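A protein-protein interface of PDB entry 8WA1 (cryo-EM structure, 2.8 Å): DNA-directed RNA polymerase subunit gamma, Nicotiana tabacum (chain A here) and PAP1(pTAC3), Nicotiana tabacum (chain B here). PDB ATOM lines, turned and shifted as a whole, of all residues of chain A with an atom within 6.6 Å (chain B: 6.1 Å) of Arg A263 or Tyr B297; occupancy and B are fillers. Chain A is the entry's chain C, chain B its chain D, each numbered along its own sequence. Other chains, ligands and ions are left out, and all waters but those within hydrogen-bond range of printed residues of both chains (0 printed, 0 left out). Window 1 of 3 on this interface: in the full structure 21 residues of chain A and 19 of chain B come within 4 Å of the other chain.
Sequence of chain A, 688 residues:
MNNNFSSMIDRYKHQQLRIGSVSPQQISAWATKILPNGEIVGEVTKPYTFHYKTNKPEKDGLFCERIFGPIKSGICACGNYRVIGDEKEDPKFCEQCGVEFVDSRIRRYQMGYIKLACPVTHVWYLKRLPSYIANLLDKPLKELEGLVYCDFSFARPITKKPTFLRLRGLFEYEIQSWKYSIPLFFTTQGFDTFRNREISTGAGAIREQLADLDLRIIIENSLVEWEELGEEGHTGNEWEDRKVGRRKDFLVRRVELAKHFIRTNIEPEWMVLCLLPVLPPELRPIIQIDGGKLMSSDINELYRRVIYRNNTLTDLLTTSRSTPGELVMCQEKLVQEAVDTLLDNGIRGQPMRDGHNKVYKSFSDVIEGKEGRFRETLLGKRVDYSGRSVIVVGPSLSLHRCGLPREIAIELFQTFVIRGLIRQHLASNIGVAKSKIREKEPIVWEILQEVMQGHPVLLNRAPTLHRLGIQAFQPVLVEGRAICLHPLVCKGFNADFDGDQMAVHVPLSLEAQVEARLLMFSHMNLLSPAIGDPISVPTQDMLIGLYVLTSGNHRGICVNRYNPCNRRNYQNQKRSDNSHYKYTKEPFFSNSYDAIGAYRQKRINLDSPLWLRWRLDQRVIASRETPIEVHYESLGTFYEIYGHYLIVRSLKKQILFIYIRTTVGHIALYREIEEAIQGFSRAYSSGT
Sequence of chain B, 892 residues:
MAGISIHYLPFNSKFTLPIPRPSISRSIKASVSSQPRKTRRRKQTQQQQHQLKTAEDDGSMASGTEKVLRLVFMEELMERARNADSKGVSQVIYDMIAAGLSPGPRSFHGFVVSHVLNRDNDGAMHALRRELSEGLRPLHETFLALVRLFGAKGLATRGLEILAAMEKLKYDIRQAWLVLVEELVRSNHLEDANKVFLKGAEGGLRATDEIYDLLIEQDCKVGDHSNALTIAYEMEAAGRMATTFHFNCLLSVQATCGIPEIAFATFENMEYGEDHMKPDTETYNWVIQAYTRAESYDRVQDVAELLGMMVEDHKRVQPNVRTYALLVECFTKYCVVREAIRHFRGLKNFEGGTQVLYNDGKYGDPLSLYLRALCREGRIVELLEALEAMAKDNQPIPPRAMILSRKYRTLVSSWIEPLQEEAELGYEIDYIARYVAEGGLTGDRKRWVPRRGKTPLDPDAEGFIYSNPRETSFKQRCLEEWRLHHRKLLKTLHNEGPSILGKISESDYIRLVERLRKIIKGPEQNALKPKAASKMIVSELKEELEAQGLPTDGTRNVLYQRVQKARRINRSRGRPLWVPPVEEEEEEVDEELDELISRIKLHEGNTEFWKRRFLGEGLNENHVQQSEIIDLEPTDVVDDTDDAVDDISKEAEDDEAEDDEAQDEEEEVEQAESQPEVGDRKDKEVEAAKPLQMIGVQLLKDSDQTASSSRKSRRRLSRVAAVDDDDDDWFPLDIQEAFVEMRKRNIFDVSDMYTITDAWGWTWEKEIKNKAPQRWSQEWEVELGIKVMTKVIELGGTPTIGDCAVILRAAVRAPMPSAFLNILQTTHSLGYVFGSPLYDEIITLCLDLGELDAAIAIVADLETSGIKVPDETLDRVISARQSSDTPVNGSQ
Hydrophobic or aromatic side chains of chain A within 4 Å of the printed part of chain B: Ile A262. Of the 12 printed residues of chain B, 7 touch a printed residue of chain A. Hydrophobic or aromatic side chains of chain B that line the printed part of chain A: Ile B465 and Tyr B466. Among the printed residues, no Asp or Glu carboxylate lies within 4 Å of a Lys or Arg side-chain nitrogen of the other chain.
Of the printed residues of chain B, Arg A263 touches Ala B294 (3.3 Å), Glu B295 (3.2 Å), Ser B296 (2.9 Å), Tyr B297 (3.2 Å) and Ile B465 (3.5 Å). Tyr B297 touches one residue of chain A. Printed residues of chain A within 4 Å of Ile B465: Arg A263. Of the printed residues of chain A, Lys B454 touches Phe A261 (2.9 Å) and Ile A266 (3.0 Å). Of the printed residues of chain B, Lys A259 touches Tyr B466. Of the printed residues of chain B, Phe A261 touches Lys B454. Printed residues of chain A within 4 Å of Tyr B466: Lys A259 (3.6 Å) and Ile A262 (3.7 Å). Ile A19 touches none of the printed residues of chain B. Arg B299 touches none of the printed residues of chain A. The nearest residue of chain B that does not touch Arg A263 is Tyr B466 (4.5 Å). The nearest printed residue of chain B that does not touch Ile A262 is Ile B465 (4.1 Å).
Among the printed residues, pairs that only touch across the chains: Lys A259 with Tyr B466, Ile A262 with Tyr B466, Arg A263 with Glu B295 and Arg A263 with Ile B465.
The side-chain amino group (NZ) of Lys B454 lies within hydrogen-bond range of the backbone carbonyl oxygen (O) of Phe A261 (2.9 Å). NZ of Lys B454 sits at hydrogen-bond distance from O of Ile A266 (3.0 Å). O of Ala B294 sits at hydrogen-bond distance from NH2 of Arg A263 (3.3 Å). The backbone carbonyl oxygen (O) of Ser B296 sits close to the backbone carbonyl oxygen (O) of Arg A263, at 2.9 Å. The guanidinium group (NH1) of Arg A263 sits at hydrogen-bond distance from the backbone carbonyl oxygen (O) of Tyr B297, 3.2 Å away.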
ATOM      1  N   ARG A  18       3.332   2.059 -30.934  1.00  0.00           N
ATOM      2  CA  ARG A  18       3.910   3.384 -30.784  1.00  0.00           C
ATOM      3  C   ARG A  18       4.282   3.930 -32.155  1.00  0.00           C
ATOM      4  O   ARG A  18       4.808   3.210 -33.005  1.00  0.00           O
ATOM      5  CB  ARG A  18       5.140   3.364 -29.870  1.00  0.00           C
ATOM      6  CG  ARG A  18       5.674   4.743 -29.529  1.00  0.00           C
ATOM      7  CD  ARG A  18       6.927   4.665 -28.675  1.00  0.00           C
ATOM      8  NE  ARG A  18       7.423   5.992 -28.320  1.00  0.00           N
ATOM      9  CZ  ARG A  18       8.259   6.703 -29.070  1.00  0.00           C
ATOM     10  NH1 ARG A  18       8.698   6.216 -30.222  1.00  0.00           N
ATOM     11  NH2 ARG A  18       8.656   7.902 -28.667  1.00  0.00           N
ATOM     12  N   ILE A  19       4.004   5.218 -32.356  1.00  0.00           N
ATOM     13  CA  ILE A  19       4.289   5.905 -33.606  1.00  0.00           C
ATOM     14  C   ILE A  19       5.009   7.209 -33.283  1.00  0.00           C
ATOM     15  O   ILE A  19       4.800   7.819 -32.234  1.00  0.00           O
ATOM     16  CB  ILE A  19       3.010   6.170 -34.430  1.00  0.00           C
ATOM     17  CG1 ILE A  19       3.358   6.643 -35.844  1.00  0.00           C
ATOM     18  CG2 ILE A  19       2.121   7.186 -33.730  1.00  0.00           C
ATOM     19  CD1 ILE A  19       2.152   6.879 -36.722  1.00  0.00           C
ATOM     20  N   LEU A 215      12.404  25.051 -25.758  1.00  0.00           N
ATOM     21  CA  LEU A 215      10.961  24.901 -25.605  1.00  0.00           C
ATOM     22  C   LEU A 215      10.461  25.577 -24.336  1.00  0.00           C
ATOM     23  O   LEU A 215       9.324  26.063 -24.291  1.00  0.00           O
ATOM     24  CB  LEU A 215      10.591  23.420 -25.609  1.00  0.00           C
ATOM     25  CG  LEU A 215      11.113  22.632 -26.810  1.00  0.00           C
ATOM     26  CD1 LEU A 215      10.814  21.152 -26.653  1.00  0.00           C
ATOM     27  CD2 LEU A 215      10.520  23.172 -28.103  1.00  0.00           C
ATOM     28  N   ALA A 258       4.963  22.479 -27.739  1.00  0.00           N
ATOM     29  CA  ALA A 258       6.245  22.522 -27.042  1.00  0.00           C
ATOM     30  C   ALA A 258       6.246  21.612 -25.818  1.00  0.00           C
ATOM     31  O   ALA A 258       7.236  20.917 -25.556  1.00  0.00           O
ATOM     32  CB  ALA A 258       6.583  23.958 -26.651  1.00  0.00           C
ATOM     33  N   LYS A 259       5.145  21.592 -25.060  1.00  0.00           N
ATOM     34  CA  LYS A 259       5.069  20.729 -23.885  1.00  0.00           C
ATOM     35  C   LYS A 259       5.146  19.259 -24.272  1.00  0.00           C
ATOM     36  O   LYS A 259       5.782  18.461 -23.573  1.00  0.00           O
ATOM     37  CB  LYS A 259       3.787  21.008 -23.102  1.00  0.00           C
ATOM     38  CG  LYS A 259       3.829  22.277 -22.266  1.00  0.00           C
ATOM     39  CD  LYS A 259       2.625  22.365 -21.342  1.00  0.00           C
ATOM     40  CE  LYS A 259       2.715  23.580 -20.433  1.00  0.00           C
ATOM     41  NZ  LYS A 259       1.561  23.660 -19.496  1.00  0.00           N
ATOM     42  N   HIS A 260       4.503  18.878 -25.378  1.00  0.00           N
ATOM     43  CA  HIS A 260       4.618  17.502 -25.846  1.00  0.00           C
ATOM     44  C   HIS A 260       6.037  17.199 -26.312  1.00  0.00           C
ATOM     45  O   HIS A 260       6.576  16.128 -26.016  1.00  0.00           O
ATOM     46  CB  HIS A 260       3.611  17.237 -26.965  1.00  0.00           C
ATOM     47  CG  HIS A 260       2.229  16.939 -26.472  1.00  0.00           C
ATOM     48  ND1 HIS A 260       1.747  15.655 -26.339  1.00  0.00           N
ATOM     49  CD2 HIS A 260       1.227  17.760 -26.075  1.00  0.00           C
ATOM     50  CE1 HIS A 260       0.507  15.697 -25.884  1.00  0.00           C
ATOM     51  NE2 HIS A 260       0.168  16.963 -25.716  1.00  0.00           N
ATOM     52  N   PHE A 261       6.665  18.140 -27.021  1.00  0.00           N
ATOM     53  CA  PHE A 261       8.029  17.927 -27.497  1.00  0.00           C
ATOM     54  C   PHE A 261       9.014  17.797 -26.342  1.00  0.00           C
ATOM     55  O   PHE A 261      10.063  17.158 -26.482  1.00  0.00           O
ATOM     56  CB  PHE A 261       8.446  19.067 -28.427  1.00  0.00           C
ATOM     57  CG  PHE A 261       8.233  18.768 -29.880  1.00  0.00           C
ATOM     58  CD1 PHE A 261       8.326  17.472 -30.353  1.00  0.00           C
ATOM     59  CD2 PHE A 261       7.941  19.783 -30.775  1.00  0.00           C
ATOM     60  CE1 PHE A 261       8.133  17.192 -31.691  1.00  0.00           C
ATOM     61  CE2 PHE A 261       7.745  19.505 -32.112  1.00  0.00           C
ATOM     62  CZ  PHE A 261       7.843  18.212 -32.571  1.00  0.00           C
ATOM     63  N   ILE A 262       8.703  18.410 -25.196  1.00  0.00           N
ATOM     64  CA  ILE A 262       9.614  18.349 -24.054  1.00  0.00           C
ATOM     65  C   ILE A 262       9.773  16.916 -23.561  1.00  0.00           C
ATOM     66  O   ILE A 262      10.888  16.466 -23.266  1.00  0.00           O
ATOM     67  CB  ILE A 262       9.125  19.280 -22.929  1.00  0.00           C
ATOM     68  CG1 ILE A 262       9.400  20.742 -23.284  1.00  0.00           C
ATOM     69  CG2 ILE A 262       9.787  18.922 -21.605  1.00  0.00           C
ATOM     70  CD1 ILE A 262       8.922  21.724 -22.237  1.00  0.00           C
ATOM     71  N   ARG A 263       8.675  16.169 -23.483  1.00  0.00           N
ATOM     72  CA  ARG A 263       8.653  14.866 -22.824  1.00  0.00           C
ATOM     73  C   ARG A 263       8.135  13.768 -23.747  1.00  0.00           C
ATOM     74  O   ARG A 263       7.260  12.984 -23.377  1.00  0.00           O
ATOM     75  CB  ARG A 263       7.815  14.925 -21.549  1.00  0.00           C
ATOM     76  CG  ARG A 263       8.581  14.577 -20.283  1.00  0.00           C
ATOM     77  CD  ARG A 263       7.693  14.697 -19.057  1.00  0.00           C
ATOM     78  NE  ARG A 263       8.412  14.389 -17.825  1.00  0.00           N
ATOM     79  CZ  ARG A 263       8.450  13.186 -17.263  1.00  0.00           C
ATOM     80  NH1 ARG A 263       7.808  12.170 -17.823  1.00  0.00           N
ATOM     81  NH2 ARG A 263       9.129  12.998 -16.140  1.00  0.00           N
ATOM     82  N   THR A 264       8.672  13.693 -24.968  1.00  0.00           N
ATOM     83  CA  THR A 264       8.276  12.634 -25.889  1.00  0.00           C
ATOM     84  C   THR A 264       9.461  11.965 -26.573  1.00  0.00           C
ATOM     85  O   THR A 264       9.245  11.161 -27.489  1.00  0.00           O
ATOM     86  CB  THR A 264       7.320  13.171 -26.959  1.00  0.00           C
ATOM     87  OG1 THR A 264       6.799  12.079 -27.726  1.00  0.00           O
ATOM     88  CG2 THR A 264       8.053  14.124 -27.892  1.00  0.00           C
ATOM     89  N   ASN A 265      10.693  12.263 -26.150  1.00  0.00           N
ATOM     90  CA  ASN A 265      11.925  11.770 -26.779  1.00  0.00           C
ATOM     91  C   ASN A 265      11.864  11.857 -28.306  1.00  0.00           C
ATOM     92  O   ASN A 265      12.394  11.006 -29.023  1.00  0.00           O
ATOM     93  CB  ASN A 265      12.269  10.347 -26.313  1.00  0.00           C
ATOM     94  CG  ASN A 265      11.259   9.304 -26.762  1.00  0.00           C
ATOM     95  OD1 ASN A 265      11.368   8.746 -27.853  1.00  0.00           O
ATOM     96  ND2 ASN A 265      10.275   9.031 -25.913  1.00  0.00           N
ATOM     97  N   ILE A 266      11.227  12.916 -28.806  1.00  0.00           N
ATOM     98  CA  ILE A 266      11.188  13.218 -30.229  1.00  0.00           C
ATOM     99  C   ILE A 266      11.641  14.660 -30.411  1.00  0.00           C
ATOM    100  O   ILE A 266      11.251  15.553 -29.653  1.00  0.00           O
ATOM    101  CB  ILE A 266       9.780  13.001 -30.838  1.00  0.00           C
ATOM    102  CG1 ILE A 266       9.325  11.553 -30.644  1.00  0.00           C
ATOM    103  CG2 ILE A 266       9.767  13.361 -32.314  1.00  0.00           C
ATOM    104  CD1 ILE A 266      10.172  10.538 -31.375  1.00  0.00           C
ATOM    105  N   GLU B 261       0.509   2.110 -16.373  1.00  0.00           N
ATOM    106  CA  GLU B 261      -0.704   1.490 -16.879  1.00  0.00           C
ATOM    107  C   GLU B 261      -0.892   0.058 -16.397  1.00  0.00           C
ATOM    108  O   GLU B 261      -2.014  -0.457 -16.464  1.00  0.00           O
ATOM    109  CB  GLU B 261      -0.716   1.517 -18.413  1.00  0.00           C
ATOM    110  CG  GLU B 261       0.259   2.514 -19.039  1.00  0.00           C
ATOM    111  CD  GLU B 261      -0.188   3.959 -18.906  1.00  0.00           C
ATOM    112  OE1 GLU B 261      -1.361   4.197 -18.546  1.00  0.00           O
ATOM    113  OE2 GLU B 261       0.637   4.859 -19.165  1.00  0.00           O
ATOM    114  N   ALA B 294       6.399   8.721 -13.122  1.00  0.00           N
ATOM    115  CA  ALA B 294       6.554   8.267 -14.493  1.00  0.00           C
ATOM    116  C   ALA B 294       7.643   9.066 -15.202  1.00  0.00           C
ATOM    117  O   ALA B 294       8.047  10.147 -14.764  1.00  0.00           O
ATOM    118  CB  ALA B 294       5.235   8.394 -15.250  1.00  0.00           C
ATOM    119  N   GLU B 295       8.123   8.514 -16.318  1.00  0.00           N
ATOM    120  CA  GLU B 295       9.214   9.112 -17.076  1.00  0.00           C
ATOM    121  C   GLU B 295       8.900   9.243 -18.562  1.00  0.00           C
ATOM    122  O   GLU B 295       9.809   9.530 -19.351  1.00  0.00           O
ATOM    123  CB  GLU B 295      10.497   8.296 -16.890  1.00  0.00           C
ATOM    124  CG  GLU B 295      10.918   8.114 -15.439  1.00  0.00           C
ATOM    125  CD  GLU B 295      12.109   7.189 -15.285  1.00  0.00           C
ATOM    126  OE1 GLU B 295      12.673   6.766 -16.316  1.00  0.00           O
ATOM    127  OE2 GLU B 295      12.480   6.881 -14.132  1.00  0.00           O
ATOM    128  N   SER B 296       7.645   9.044 -18.969  1.00  0.00           N
ATOM    129  CA  SER B 296       7.305   8.970 -20.381  1.00  0.00           C
ATOM    130  C   SER B 296       6.381  10.074 -20.876  1.00  0.00           C
ATOM    131  O   SER B 296       6.582  10.556 -21.994  1.00  0.00           O
ATOM    132  CB  SER B 296       6.657   7.615 -20.704  1.00  0.00           C
ATOM    133  OG  SER B 296       7.530   6.544 -20.386  1.00  0.00           O
ATOM    134  N   TYR B 297       5.389  10.488 -20.093  1.00  0.00           N
ATOM    135  CA  TYR B 297       4.409  11.456 -20.569  1.00  0.00           C
ATOM    136  C   TYR B 297       4.004  12.363 -19.411  1.00  0.00           C
ATOM    137  O   TYR B 297       4.643  12.375 -18.354  1.00  0.00           O
ATOM    138  CB  TYR B 297       3.203  10.744 -21.195  1.00  0.00           C
ATOM    139  CG  TYR B 297       3.518  10.033 -22.491  1.00  0.00           C
ATOM    140  CD1 TYR B 297       3.579  10.730 -23.690  1.00  0.00           C
ATOM    141  CD2 TYR B 297       3.751   8.665 -22.516  1.00  0.00           C
ATOM    142  CE1 TYR B 297       3.867  10.085 -24.877  1.00  0.00           C
ATOM    143  CE2 TYR B 297       4.040   8.010 -23.697  1.00  0.00           C
ATOM    144  CZ  TYR B 297       4.097   8.725 -24.875  1.00  0.00           C
ATOM    145  OH  TYR B 297       4.383   8.078 -26.054  1.00  0.00           O
ATOM    146  N   ASP B 298       2.932  13.127 -19.622  1.00  0.00           N
ATOM    147  CA  ASP B 298       2.520  14.129 -18.643  1.00  0.00           C
ATOM    148  C   ASP B 298       2.026  13.473 -17.359  1.00  0.00           C
ATOM    149  O   ASP B 298       2.633  13.632 -16.295  1.00  0.00           O
ATOM    150  CB  ASP B 298       1.439  15.025 -19.246  1.00  0.00           C
ATOM    151  CG  ASP B 298       1.267  16.327 -18.490  1.00  0.00           C
ATOM    152  OD1 ASP B 298       2.024  16.559 -17.525  1.00  0.00           O
ATOM    153  OD2 ASP B 298       0.378  17.120 -18.865  1.00  0.00           O
ATOM    154  N   ARG B 299       0.929  12.718 -17.445  1.00  0.00           N
ATOM    155  CA  ARG B 299       0.363  11.996 -16.303  1.00  0.00           C
ATOM    156  C   ARG B 299       0.043  12.924 -15.134  1.00  0.00           C
ATOM    157  O   ARG B 299       0.316  12.597 -13.976  1.00  0.00           O
ATOM    158  CB  ARG B 299       1.288  10.863 -15.840  1.00  0.00           C
ATOM    159  CG  ARG B 299       1.131   9.558 -16.609  1.00  0.00           C
ATOM    160  CD  ARG B 299       1.613   9.681 -18.044  1.00  0.00           C
ATOM    161  NE  ARG B 299       1.617   8.395 -18.733  1.00  0.00           N
ATOM    162  CZ  ARG B 299       2.661   7.574 -18.770  1.00  0.00           C
ATOM    163  NH1 ARG B 299       3.789   7.907 -18.159  1.00  0.00           N
ATOM    164  NH2 ARG B 299       2.580   6.422 -19.420  1.00  0.00           N
ATOM    165  N   TYR B 334       4.787  19.365 -11.192  1.00  0.00           N
ATOM    166  CA  TYR B 334       4.045  19.953 -12.298  1.00  0.00           C
ATOM    167  C   TYR B 334       3.672  21.412 -12.054  1.00  0.00           C
ATOM    168  O   TYR B 334       2.762  21.924 -12.713  1.00  0.00           O
ATOM    169  CB  TYR B 334       2.789  19.129 -12.587  1.00  0.00           C
ATOM    170  CG  TYR B 334       3.094  17.736 -13.085  1.00  0.00           C
ATOM    171  CD1 TYR B 334       3.366  17.503 -14.426  1.00  0.00           C
ATOM    172  CD2 TYR B 334       3.125  16.658 -12.214  1.00  0.00           C
ATOM    173  CE1 TYR B 334       3.650  16.233 -14.883  1.00  0.00           C
ATOM    174  CE2 TYR B 334       3.409  15.384 -12.662  1.00  0.00           C
ATOM    175  CZ  TYR B 334       3.672  15.178 -13.998  1.00  0.00           C
ATOM    176  OH  TYR B 334       3.955  13.910 -14.449  1.00  0.00           O
ATOM    177  N   LYS B 454      17.933  18.796 -25.615  1.00  0.00           N
ATOM    178  CA  LYS B 454      16.819  19.132 -24.726  1.00  0.00           C
ATOM    179  C   LYS B 454      17.209  18.812 -23.282  1.00  0.00           C
ATOM    180  O   LYS B 454      16.701  17.886 -22.647  1.00  0.00           O
ATOM    181  CB  LYS B 454      15.557  18.392 -25.145  1.00  0.00           C
ATOM    182  CG  LYS B 454      15.057  18.750 -26.535  1.00  0.00           C
ATOM    183  CD  LYS B 454      13.746  18.047 -26.850  1.00  0.00           C
ATOM    184  CE  LYS B 454      13.885  16.538 -26.738  1.00  0.00           C
ATOM    185  NZ  LYS B 454      12.598  15.843 -27.012  1.00  0.00           N
ATOM    186  N   PHE B 464      11.955  18.892 -11.990  1.00  0.00           N
ATOM    187  CA  PHE B 464      10.646  19.277 -12.491  1.00  0.00           C
ATOM    188  C   PHE B 464      10.394  18.659 -13.860  1.00  0.00           C
ATOM    189  O   PHE B 464      11.321  18.426 -14.640  1.00  0.00           O
ATOM    190  CB  PHE B 464      10.525  20.801 -12.566  1.00  0.00           C
ATOM    191  CG  PHE B 464      10.493  21.470 -11.221  1.00  0.00           C
ATOM    192  CD1 PHE B 464      11.666  21.758 -10.545  1.00  0.00           C
ATOM    193  CD2 PHE B 464       9.285  21.808 -10.632  1.00  0.00           C
ATOM    194  CE1 PHE B 464      11.636  22.371  -9.307  1.00  0.00           C
ATOM    195  CE2 PHE B 464       9.250  22.423  -9.395  1.00  0.00           C
ATOM    196  CZ  PHE B 464      10.427  22.704  -8.733  1.00  0.00           C
ATOM    197  N   ILE B 465       9.118  18.388 -14.142  1.00  0.00           N
ATOM    198  CA  ILE B 465       8.757  17.692 -15.375  1.00  0.00           C
ATOM    199  C   ILE B 465       9.020  18.573 -16.590  1.00  0.00           C
ATOM    200  O   ILE B 465       9.538  18.106 -17.612  1.00  0.00           O
ATOM    201  CB  ILE B 465       7.291  17.221 -15.310  1.00  0.00           C
ATOM    202  CG1 ILE B 465       7.212  15.772 -14.821  1.00  0.00           C
ATOM    203  CG2 ILE B 465       6.608  17.354 -16.665  1.00  0.00           C
ATOM    204  CD1 ILE B 465       7.774  15.549 -13.437  1.00  0.00           C
ATOM    205  N   TYR B 466       8.684  19.857 -16.499  1.00  0.00           N
ATOM    206  CA  TYR B 466       8.855  20.781 -17.613  1.00  0.00           C
ATOM    207  C   TYR B 466       9.926  21.826 -17.351  1.00  0.00           C
ATOM    208  O   TYR B 466      10.878  21.941 -18.134  1.00  0.00           O
ATOM    209  CB  TYR B 466       7.522  21.479 -17.933  1.00  0.00           C
ATOM    210  CG  TYR B 466       6.487  20.580 -18.566  1.00  0.00           C
ATOM    211  CD1 TYR B 466       6.859  19.569 -19.442  1.00  0.00           C
ATOM    212  CD2 TYR B 466       5.138  20.743 -18.288  1.00  0.00           C
ATOM    213  CE1 TYR B 466       5.914  18.746 -20.023  1.00  0.00           C
ATOM    214  CE2 TYR B 466       4.186  19.925 -18.864  1.00  0.00           C
ATOM    215  CZ  TYR B 466       4.579  18.929 -19.730  1.00  0.00           C
ATOM    216  OH  TYR B 466       3.634  18.111 -20.305  1.00  0.00           O
